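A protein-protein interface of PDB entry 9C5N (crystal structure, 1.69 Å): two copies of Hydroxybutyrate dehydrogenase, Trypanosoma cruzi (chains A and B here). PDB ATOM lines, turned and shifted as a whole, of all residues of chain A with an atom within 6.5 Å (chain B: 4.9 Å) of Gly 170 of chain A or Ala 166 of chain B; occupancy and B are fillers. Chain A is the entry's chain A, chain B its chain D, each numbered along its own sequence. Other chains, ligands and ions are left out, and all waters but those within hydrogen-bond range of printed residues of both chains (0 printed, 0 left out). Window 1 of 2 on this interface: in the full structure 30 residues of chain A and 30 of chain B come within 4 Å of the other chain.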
ATOM      1  N   ASN A 123      19.149 -16.257  15.733  1.00  0.00           N
ATOM      2  CA  ASN A 123      20.014 -16.902  14.767  1.00  0.00           C
ATOM      3  C   ASN A 123      20.358 -15.997  13.599  1.00  0.00           C
ATOM      4  O   ASN A 123      21.278 -16.326  12.844  1.00  0.00           O
ATOM      5  CB  ASN A 123      19.357 -18.168  14.195  1.00  0.00           C
ATOM      6  CG  ASN A 123      19.318 -19.316  15.174  1.00  0.00           C
ATOM      7  OD1 ASN A 123      18.330 -19.521  15.863  1.00  0.00           O
ATOM      8  ND2 ASN A 123      20.382 -20.096  15.211  1.00  0.00           N
ATOM      9  N   LEU A 124      19.586 -14.921  13.382  1.00  0.00           N
ATOM     10  CA  LEU A 124      19.843 -14.006  12.279  1.00  0.00           C
ATOM     11  C   LEU A 124      19.975 -12.546  12.686  1.00  0.00           C
ATOM     12  O   LEU A 124      21.007 -11.914  12.441  1.00  0.00           O
ATOM     13  CB  LEU A 124      18.724 -14.138  11.238  1.00  0.00           C
ATOM     14  CG  LEU A 124      18.760 -13.175  10.064  1.00  0.00           C
ATOM     15  CD1 LEU A 124      20.094 -13.196   9.343  1.00  0.00           C
ATOM     16  CD2 LEU A 124      17.650 -13.559   9.097  1.00  0.00           C
ATOM     17  N   GLY A 154      21.633 -24.158   6.663  1.00  0.00           N
ATOM     18  CA  GLY A 154      21.672 -22.918   5.911  1.00  0.00           C
ATOM     19  C   GLY A 154      21.904 -23.107   4.432  1.00  0.00           C
ATOM     20  O   GLY A 154      21.828 -22.141   3.663  1.00  0.00           O
ATOM     21  N   CYS A 165      16.069 -23.548   9.452  1.00  0.00           N
ATOM     22  CA  CYS A 165      16.608 -23.518   8.095  1.00  0.00           C
ATOM     23  C   CYS A 165      16.459 -22.133   7.477  1.00  0.00           C
ATOM     24  O   CYS A 165      17.381 -21.630   6.817  1.00  0.00           O
ATOM     25  CB  CYS A 165      15.913 -24.566   7.219  1.00  0.00           C
ATOM     26  SG  CYS A 165      16.317 -26.266   7.586  1.00  0.00           S
ATOM     27  N   ALA A 166      15.314 -21.485   7.700  1.00  0.00           N
ATOM     28  CA  ALA A 166      15.150 -20.123   7.205  1.00  0.00           C
ATOM     29  C   ALA A 166      16.187 -19.180   7.818  1.00  0.00           C
ATOM     30  O   ALA A 166      16.838 -18.403   7.109  1.00  0.00           O
ATOM     31  CB  ALA A 166      13.739 -19.625   7.493  1.00  0.00           C
ATOM     32  N   ALA A 167      16.366 -19.239   9.139  1.00  0.00           N
ATOM     33  CA  ALA A 167      17.299 -18.332   9.797  1.00  0.00           C
ATOM     34  C   ALA A 167      18.736 -18.572   9.356  1.00  0.00           C
ATOM     35  O   ALA A 167      19.493 -17.618   9.136  1.00  0.00           O
ATOM     36  CB  ALA A 167      17.169 -18.495  11.306  1.00  0.00           C
ATOM     37  N   LYS A 168      19.145 -19.836   9.268  1.00  0.00           N
ATOM     38  CA  LYS A 168      20.516 -20.156   8.903  1.00  0.00           C
ATOM     39  C   LYS A 168      20.777 -19.872   7.430  1.00  0.00           C
ATOM     40  O   LYS A 168      21.866 -19.405   7.083  1.00  0.00           O
ATOM     41  CB  LYS A 168      20.823 -21.608   9.241  1.00  0.00           C
ATOM     42  CG  LYS A 168      20.796 -21.930  10.728  1.00  0.00           C
ATOM     43  CD  LYS A 168      21.858 -21.179  11.506  1.00  0.00           C
ATOM     44  CE  LYS A 168      22.059 -21.842  12.869  1.00  0.00           C
ATOM     45  NZ  LYS A 168      23.063 -21.123  13.719  1.00  0.00           N
ATOM     46  N   HIS A 169      19.781 -20.076   6.559  1.00  0.00           N
ATOM     47  CA  HIS A 169      19.920 -19.628   5.178  1.00  0.00           C
ATOM     48  C   HIS A 169      20.108 -18.118   5.143  1.00  0.00           C
ATOM     49  O   HIS A 169      20.970 -17.597   4.420  1.00  0.00           O
ATOM     50  CB  HIS A 169      18.691 -20.002   4.315  1.00  0.00           C
ATOM     51  CG  HIS A 169      18.753 -21.371   3.685  1.00  0.00           C
ATOM     52  ND1 HIS A 169      18.639 -22.531   4.421  1.00  0.00           N
ATOM     53  CD2 HIS A 169      18.870 -21.763   2.390  1.00  0.00           C
ATOM     54  CE1 HIS A 169      18.723 -23.577   3.613  1.00  0.00           C
ATOM     55  NE2 HIS A 169      18.849 -23.140   2.375  1.00  0.00           N
ATOM     56  N   GLY A 170      19.300 -17.402   5.932  1.00  0.00           N
ATOM     57  CA  GLY A 170      19.401 -15.949   5.969  1.00  0.00           C
ATOM     58  C   GLY A 170      20.749 -15.477   6.477  1.00  0.00           C
ATOM     59  O   GLY A 170      21.296 -14.487   5.990  1.00  0.00           O
ATOM     60  N   LEU A 171      21.295 -16.169   7.476  1.00  0.00           N
ATOM     61  CA  LEU A 171      22.607 -15.814   8.007  1.00  0.00           C
ATOM     62  C   LEU A 171      23.701 -15.969   6.951  1.00  0.00           C
ATOM     63  O   LEU A 171      24.652 -15.170   6.908  1.00  0.00           O
ATOM     64  CB  LEU A 171      22.896 -16.682   9.238  1.00  0.00           C
ATOM     65  CG  LEU A 171      24.194 -16.363   9.973  1.00  0.00           C
ATOM     66  CD1 LEU A 171      24.236 -14.964  10.526  1.00  0.00           C
ATOM     67  CD2 LEU A 171      24.412 -17.411  11.097  1.00  0.00           C
ATOM     68  N   ILE A 172      23.577 -16.988   6.089  1.00  0.00           N
ATOM     69  CA  ILE A 172      24.517 -17.158   4.982  1.00  0.00           C
ATOM     70  C   ILE A 172      24.367 -16.036   3.952  1.00  0.00           C
ATOM     71  O   ILE A 172      25.370 -15.484   3.481  1.00  0.00           O
ATOM     72  CB  ILE A 172      24.342 -18.557   4.362  1.00  0.00           C
ATOM     73  CG1 ILE A 172      24.914 -19.594   5.349  1.00  0.00           C
ATOM     74  CG2 ILE A 172      25.042 -18.652   3.010  1.00  0.00           C
ATOM     75  CD1 ILE A 172      24.660 -21.001   4.975  1.00  0.00           C
ATOM     76  N   GLY A 173      23.128 -15.629   3.639  1.00  0.00           N
ATOM     77  CA  GLY A 173      22.949 -14.483   2.752  1.00  0.00           C
ATOM     78  C   GLY A 173      23.549 -13.211   3.323  1.00  0.00           C
ATOM     79  O   GLY A 173      24.211 -12.445   2.618  1.00  0.00           O
ATOM     80  N   PHE A 174      23.360 -12.996   4.626  1.00  0.00           N
ATOM     81  CA  PHE A 174      23.942 -11.849   5.310  1.00  0.00           C
ATOM     82  C   PHE A 174      25.461 -11.854   5.206  1.00  0.00           C
ATOM     83  O   PHE A 174      26.085 -10.810   4.945  1.00  0.00           O
ATOM     84  CB  PHE A 174      23.498 -11.856   6.780  1.00  0.00           C
ATOM     85  CG  PHE A 174      24.044 -10.709   7.584  1.00  0.00           C
ATOM     86  CD1 PHE A 174      23.670  -9.414   7.275  1.00  0.00           C
ATOM     87  CD2 PHE A 174      24.933 -10.907   8.635  1.00  0.00           C
ATOM     88  CE1 PHE A 174      24.190  -8.328   8.001  1.00  0.00           C
ATOM     89  CE2 PHE A 174      25.459  -9.806   9.359  1.00  0.00           C
ATOM     90  CZ  PHE A 174      25.073  -8.541   9.048  1.00  0.00           C
ATOM     91  N   THR A 175      26.064 -13.028   5.420  1.00  0.00           N
ATOM     92  CA  THR A 175      27.503 -13.201   5.343  1.00  0.00           C
ATOM     93  C   THR A 175      28.036 -12.731   4.013  1.00  0.00           C
ATOM     94  O   THR A 175      29.056 -12.024   3.946  1.00  0.00           O
ATOM     95  CB  THR A 175      27.820 -14.682   5.558  1.00  0.00           C
ATOM     96  OG1 THR A 175      27.361 -15.084   6.861  1.00  0.00           O
ATOM     97  CG2 THR A 175      29.320 -14.955   5.463  1.00  0.00           C
ATOM     98  N   VAL A 177      26.760 -10.521   1.931  1.00  0.00           N
ATOM     99  CA  VAL A 177      26.678  -9.073   1.756  1.00  0.00           C
ATOM    100  C   VAL A 177      27.759  -8.359   2.563  1.00  0.00           C
ATOM    101  O   VAL A 177      28.400  -7.422   2.072  1.00  0.00           O
ATOM    102  CB  VAL A 177      25.282  -8.555   2.125  1.00  0.00           C
ATOM    103  CG1 VAL A 177      25.284  -7.048   2.026  1.00  0.00           C
ATOM    104  CG2 VAL A 177      24.236  -9.120   1.167  1.00  0.00           C
ATOM    105  N   TRP B 116      15.348  -3.201   8.670  1.00  0.00           N
ATOM    106  CA  TRP B 116      15.778  -4.599   8.734  1.00  0.00           C
ATOM    107  C   TRP B 116      14.609  -5.479   9.166  1.00  0.00           C
ATOM    108  O   TRP B 116      14.242  -6.441   8.480  1.00  0.00           O
ATOM    109  CB  TRP B 116      16.965  -4.759   9.711  1.00  0.00           C
ATOM    110  CG  TRP B 116      17.362  -6.232   9.910  1.00  0.00           C
ATOM    111  CD1 TRP B 116      16.780  -7.116  10.766  1.00  0.00           C
ATOM    112  CD2 TRP B 116      18.388  -6.970   9.218  1.00  0.00           C
ATOM    113  NE1 TRP B 116      17.367  -8.346  10.653  1.00  0.00           N
ATOM    114  CE2 TRP B 116      18.359  -8.288   9.714  1.00  0.00           C
ATOM    115  CE3 TRP B 116      19.331  -6.642   8.246  1.00  0.00           C
ATOM    116  CZ2 TRP B 116      19.232  -9.282   9.266  1.00  0.00           C
ATOM    117  CZ3 TRP B 116      20.209  -7.630   7.803  1.00  0.00           C
ATOM    118  CH2 TRP B 116      20.151  -8.931   8.318  1.00  0.00           C
ATOM    119  N   ILE B 120      12.567  -8.479   6.921  1.00  0.00           N
ATOM    120  CA  ILE B 120      12.455  -9.866   7.378  1.00  0.00           C
ATOM    121  C   ILE B 120      10.982 -10.241   7.546  1.00  0.00           C
ATOM    122  O   ILE B 120      10.529 -11.302   7.099  1.00  0.00           O
ATOM    123  CB  ILE B 120      13.213 -10.063   8.708  1.00  0.00           C
ATOM    124  CG1 ILE B 120      14.716  -9.776   8.586  1.00  0.00           C
ATOM    125  CG2 ILE B 120      12.937 -11.459   9.298  1.00  0.00           C
ATOM    126  CD1 ILE B 120      15.418 -10.485   7.503  1.00  0.00           C
ATOM    127  N   LYS B 161      22.454  -4.509   0.352  1.00  0.00           N
ATOM    128  CA  LYS B 161      21.163  -5.177   0.412  1.00  0.00           C
ATOM    129  C   LYS B 161      21.185  -6.292   1.449  1.00  0.00           C
ATOM    130  O   LYS B 161      20.609  -7.362   1.246  1.00  0.00           O
ATOM    131  CB  LYS B 161      20.767  -5.698  -0.971  1.00  0.00           C
ATOM    132  CG  LYS B 161      20.493  -4.546  -1.951  1.00  0.00           C
ATOM    133  CD  LYS B 161      20.127  -5.034  -3.365  1.00  0.00           C
ATOM    134  CE  LYS B 161      19.819  -3.838  -4.283  1.00  0.00           C
ATOM    135  NZ  LYS B 161      19.621  -4.236  -5.706  1.00  0.00           N
ATOM    136  N   SER B 162      21.780  -6.029   2.618  1.00  0.00           N
ATOM    137  CA  SER B 162      21.917  -7.090   3.620  1.00  0.00           C
ATOM    138  C   SER B 162      20.563  -7.662   4.067  1.00  0.00           C
ATOM    139  O   SER B 162      20.393  -8.885   4.126  1.00  0.00           O
ATOM    140  CB  SER B 162      22.719  -6.565   4.816  1.00  0.00           C
ATOM    141  OG  SER B 162      22.144  -5.411   5.403  1.00  0.00           O
ATOM    142  N   ALA B 163      19.598  -6.812   4.422  1.00  0.00           N
ATOM    143  CA  ALA B 163      18.328  -7.345   4.921  1.00  0.00           C
ATOM    144  C   ALA B 163      17.599  -8.132   3.844  1.00  0.00           C
ATOM    145  O   ALA B 163      17.020  -9.196   4.107  1.00  0.00           O
ATOM    146  CB  ALA B 163      17.437  -6.215   5.426  1.00  0.00           C
ATOM    147  N   TYR B 164      17.594  -7.602   2.629  1.00  0.00           N
ATOM    148  CA  TYR B 164      16.869  -8.238   1.537  1.00  0.00           C
ATOM    149  C   TYR B 164      17.495  -9.570   1.161  1.00  0.00           C
ATOM    150  O   TYR B 164      16.782 -10.572   0.996  1.00  0.00           O
ATOM    151  CB  TYR B 164      16.858  -7.274   0.365  1.00  0.00           C
ATOM    152  CG  TYR B 164      16.000  -7.649  -0.808  1.00  0.00           C
ATOM    153  CD1 TYR B 164      14.667  -7.241  -0.880  1.00  0.00           C
ATOM    154  CD2 TYR B 164      16.536  -8.358  -1.877  1.00  0.00           C
ATOM    155  CE1 TYR B 164      13.896  -7.536  -1.999  1.00  0.00           C
ATOM    156  CE2 TYR B 164      15.771  -8.665  -2.986  1.00  0.00           C
ATOM    157  CZ  TYR B 164      14.456  -8.243  -3.043  1.00  0.00           C
ATOM    158  OH  TYR B 164      13.702  -8.557  -4.151  1.00  0.00           O
ATOM    159  N   CYS B 165      18.827  -9.617   1.061  1.00  0.00           N
ATOM    160  CA  CYS B 165      19.508 -10.881   0.780  1.00  0.00           C
ATOM    161  C   CYS B 165      19.296 -11.886   1.908  1.00  0.00           C
ATOM    162  O   CYS B 165      19.052 -13.078   1.661  1.00  0.00           O
ATOM    163  CB  CYS B 165      21.003 -10.634   0.548  1.00  0.00           C
ATOM    164  SG  CYS B 165      21.417  -9.770  -0.976  1.00  0.00           S
ATOM    165  N   ALA B 166      19.321 -11.425   3.159  1.00  0.00           N
ATOM    166  CA  ALA B 166      19.049 -12.345   4.256  1.00  0.00           C
ATOM    167  C   ALA B 166      17.626 -12.882   4.181  1.00  0.00           C
ATOM    168  O   ALA B 166      17.397 -14.085   4.333  1.00  0.00           O
ATOM    169  CB  ALA B 166      19.288 -11.659   5.597  1.00  0.00           C
ATOM    170  N   ALA B 167      16.651 -11.998   3.949  1.00  0.00           N
ATOM    171  CA  ALA B 167      15.258 -12.435   3.945  1.00  0.00           C
ATOM    172  C   ALA B 167      14.987 -13.373   2.774  1.00  0.00           C
ATOM    173  O   ALA B 167      14.268 -14.364   2.912  1.00  0.00           O
ATOM    174  CB  ALA B 167      14.335 -11.228   3.866  1.00  0.00           C
ATOM    175  N   LYS B 168      15.552 -13.070   1.607  1.00  0.00           N
ATOM    176  CA  LYS B 168      15.296 -13.890   0.424  1.00  0.00           C
ATOM    177  C   LYS B 168      16.025 -15.228   0.506  1.00  0.00           C
ATOM    178  O   LYS B 168      15.494 -16.254   0.062  1.00  0.00           O
ATOM    179  CB  LYS B 168      15.684 -13.114  -0.836  1.00  0.00           C
ATOM    180  CG  LYS B 168      14.800 -11.871  -1.098  1.00  0.00           C
ATOM    181  CD  LYS B 168      13.330 -12.222  -1.387  1.00  0.00           C
ATOM    182  CE  LYS B 168      12.601 -11.021  -2.019  1.00  0.00           C
ATOM    183  NZ  LYS B 168      11.140 -11.285  -2.282  1.00  0.00           N
ATOM    184  N   HIS B 169      17.240 -15.247   1.070  1.00  0.00           N
ATOM    185  CA  HIS B 169      17.893 -16.515   1.377  1.00  0.00           C
ATOM    186  C   HIS B 169      17.018 -17.330   2.330  1.00  0.00           C
ATOM    187  O   HIS B 169      16.807 -18.523   2.130  1.00  0.00           O
ATOM    188  CB  HIS B 169      19.286 -16.280   2.009  1.00  0.00           C
ATOM    189  CG  HIS B 169      20.419 -16.125   1.023  1.00  0.00           C
ATOM    190  ND1 HIS B 169      20.579 -14.999   0.239  1.00  0.00           N
ATOM    191  CD2 HIS B 169      21.478 -16.928   0.740  1.00  0.00           C
ATOM    192  CE1 HIS B 169      21.664 -15.132  -0.509  1.00  0.00           C
ATOM    193  NE2 HIS B 169      22.231 -16.292  -0.221  1.00  0.00           N
ATOM    194  N   GLY B 170      16.498 -16.690   3.374  1.00  0.00           N
ATOM    195  CA  GLY B 170      15.659 -17.394   4.327  1.00  0.00           C
ATOM    196  C   GLY B 170      14.396 -17.955   3.704  1.00  0.00           C
ATOM    197  O   GLY B 170      13.976 -19.063   4.032  1.00  0.00           O
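The backbone carbonyl oxygen (O) of Cys 165 of chain B sits at hydrogen-bond distance from a ring nitrogen (ND1) of His 169 of chain B, 2.8 Å away. O of Lys 161 of chain B lies close to SG of Cys 165 of chain B, at 3.4 Å. A ring nitrogen (ND1) of His 169 of chain A lies close to the backbone carbonyl oxygen (O) of Gly 154 of chain A. The backbone carbonyl oxygen (O) of Cys 165 of chain A is in hydrogen-bond range of a ring nitrogen (ND1) of His 169 of chain A (2.9 Å).
Of chain B, only Ala 166, His 169 and Gly 170 come within 4 Å of Gly 170 of chain A. Of chain A, only Gly 170 comes within 4 Å of Ala 166 of chain B. Of the printed residues of chain A, Ser 162 of chain B touches Phe 174 and Val 177. Printed residues of chain A within 4 Å of Trp 116 of chain B: Phe 174. Printed residues of chain B within 4 Å of Val 177 of chain A: Ser 162 (3.7 Å) and Cys 165 (3.6 Å). Of the printed residues of chain B, Gly 173 of chain A touches His 169. Printed residues of chain A within 4 Å of Cys 165 of chain B: Val 177 (3.6 Å). Ala 167 of chain A touches none of the printed residues of chain B. The nearest residue of chain A that does not touch Ala 166 of chain B is Leu 124 of chain A (4.1 Å).
Ala 166 of chain A touches Gly 170 of chain B, and with the chains exchanged Gly 170 of chain A touches Ala 166 of chain B. His 169 of chain B touches its own counterpart, His 169 of chain A. His 169 of chain A touches Gly 170 of chain B, and with the chains exchanged Gly 170 of chain A touches His 169 of chain B. Gly 170 of chain A touches its own counterpart, Gly 170 of chain B. Of the 11 pairs that touch across the chains among the printed residues, 6 have their exchanged pair printed and touching as well.
Among the printed residues, merely in contact across the chains: Ala 166 of chain A with Gly 170 of chain B, Gly 170 of chain A with Ala 166 of chain B, His 169 of chain A with His 169 of chain B, Gly 173 of chain A with His 169 of chain B, Val 177 of chain A with Cys 165 of chain B, Val 177 of chain A with Ser 162 of chain B, Phe 174 of chain A with Trp 116 of chain B, Gly 170 of chain A with Gly 170 of chain B, Phe 174 of chain A with Ser 162 of chain B, Gly 170 of chain A with His 169 of chain B and His 169 of chain A with Gly 170 of chain B.
Printed residues of chain B that touch a printed residue of chain A: Trp 116, Ser 162, Cys 165, Ala 166, His 169 and Gly 170. Hydrophobic or aromatic side chains of chain B within 4 Å of the printed part of chain A: Trp 116, Ala 166 and His 169. Of the 15 printed residues of chain A, 6 touch a printed residue of chain B. Printed residues of chain A that touch a printed residue of chain B: Ala 166, His 169, Gly 170, Gly 173, Phe 174 and Val 177. Among the printed residues, 11 pairs touch across the chains. Among the printed residues, no Asp or Glu carboxylate lies within 4 Å of a Lys or Arg side-chain nitrogen of the other chain.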
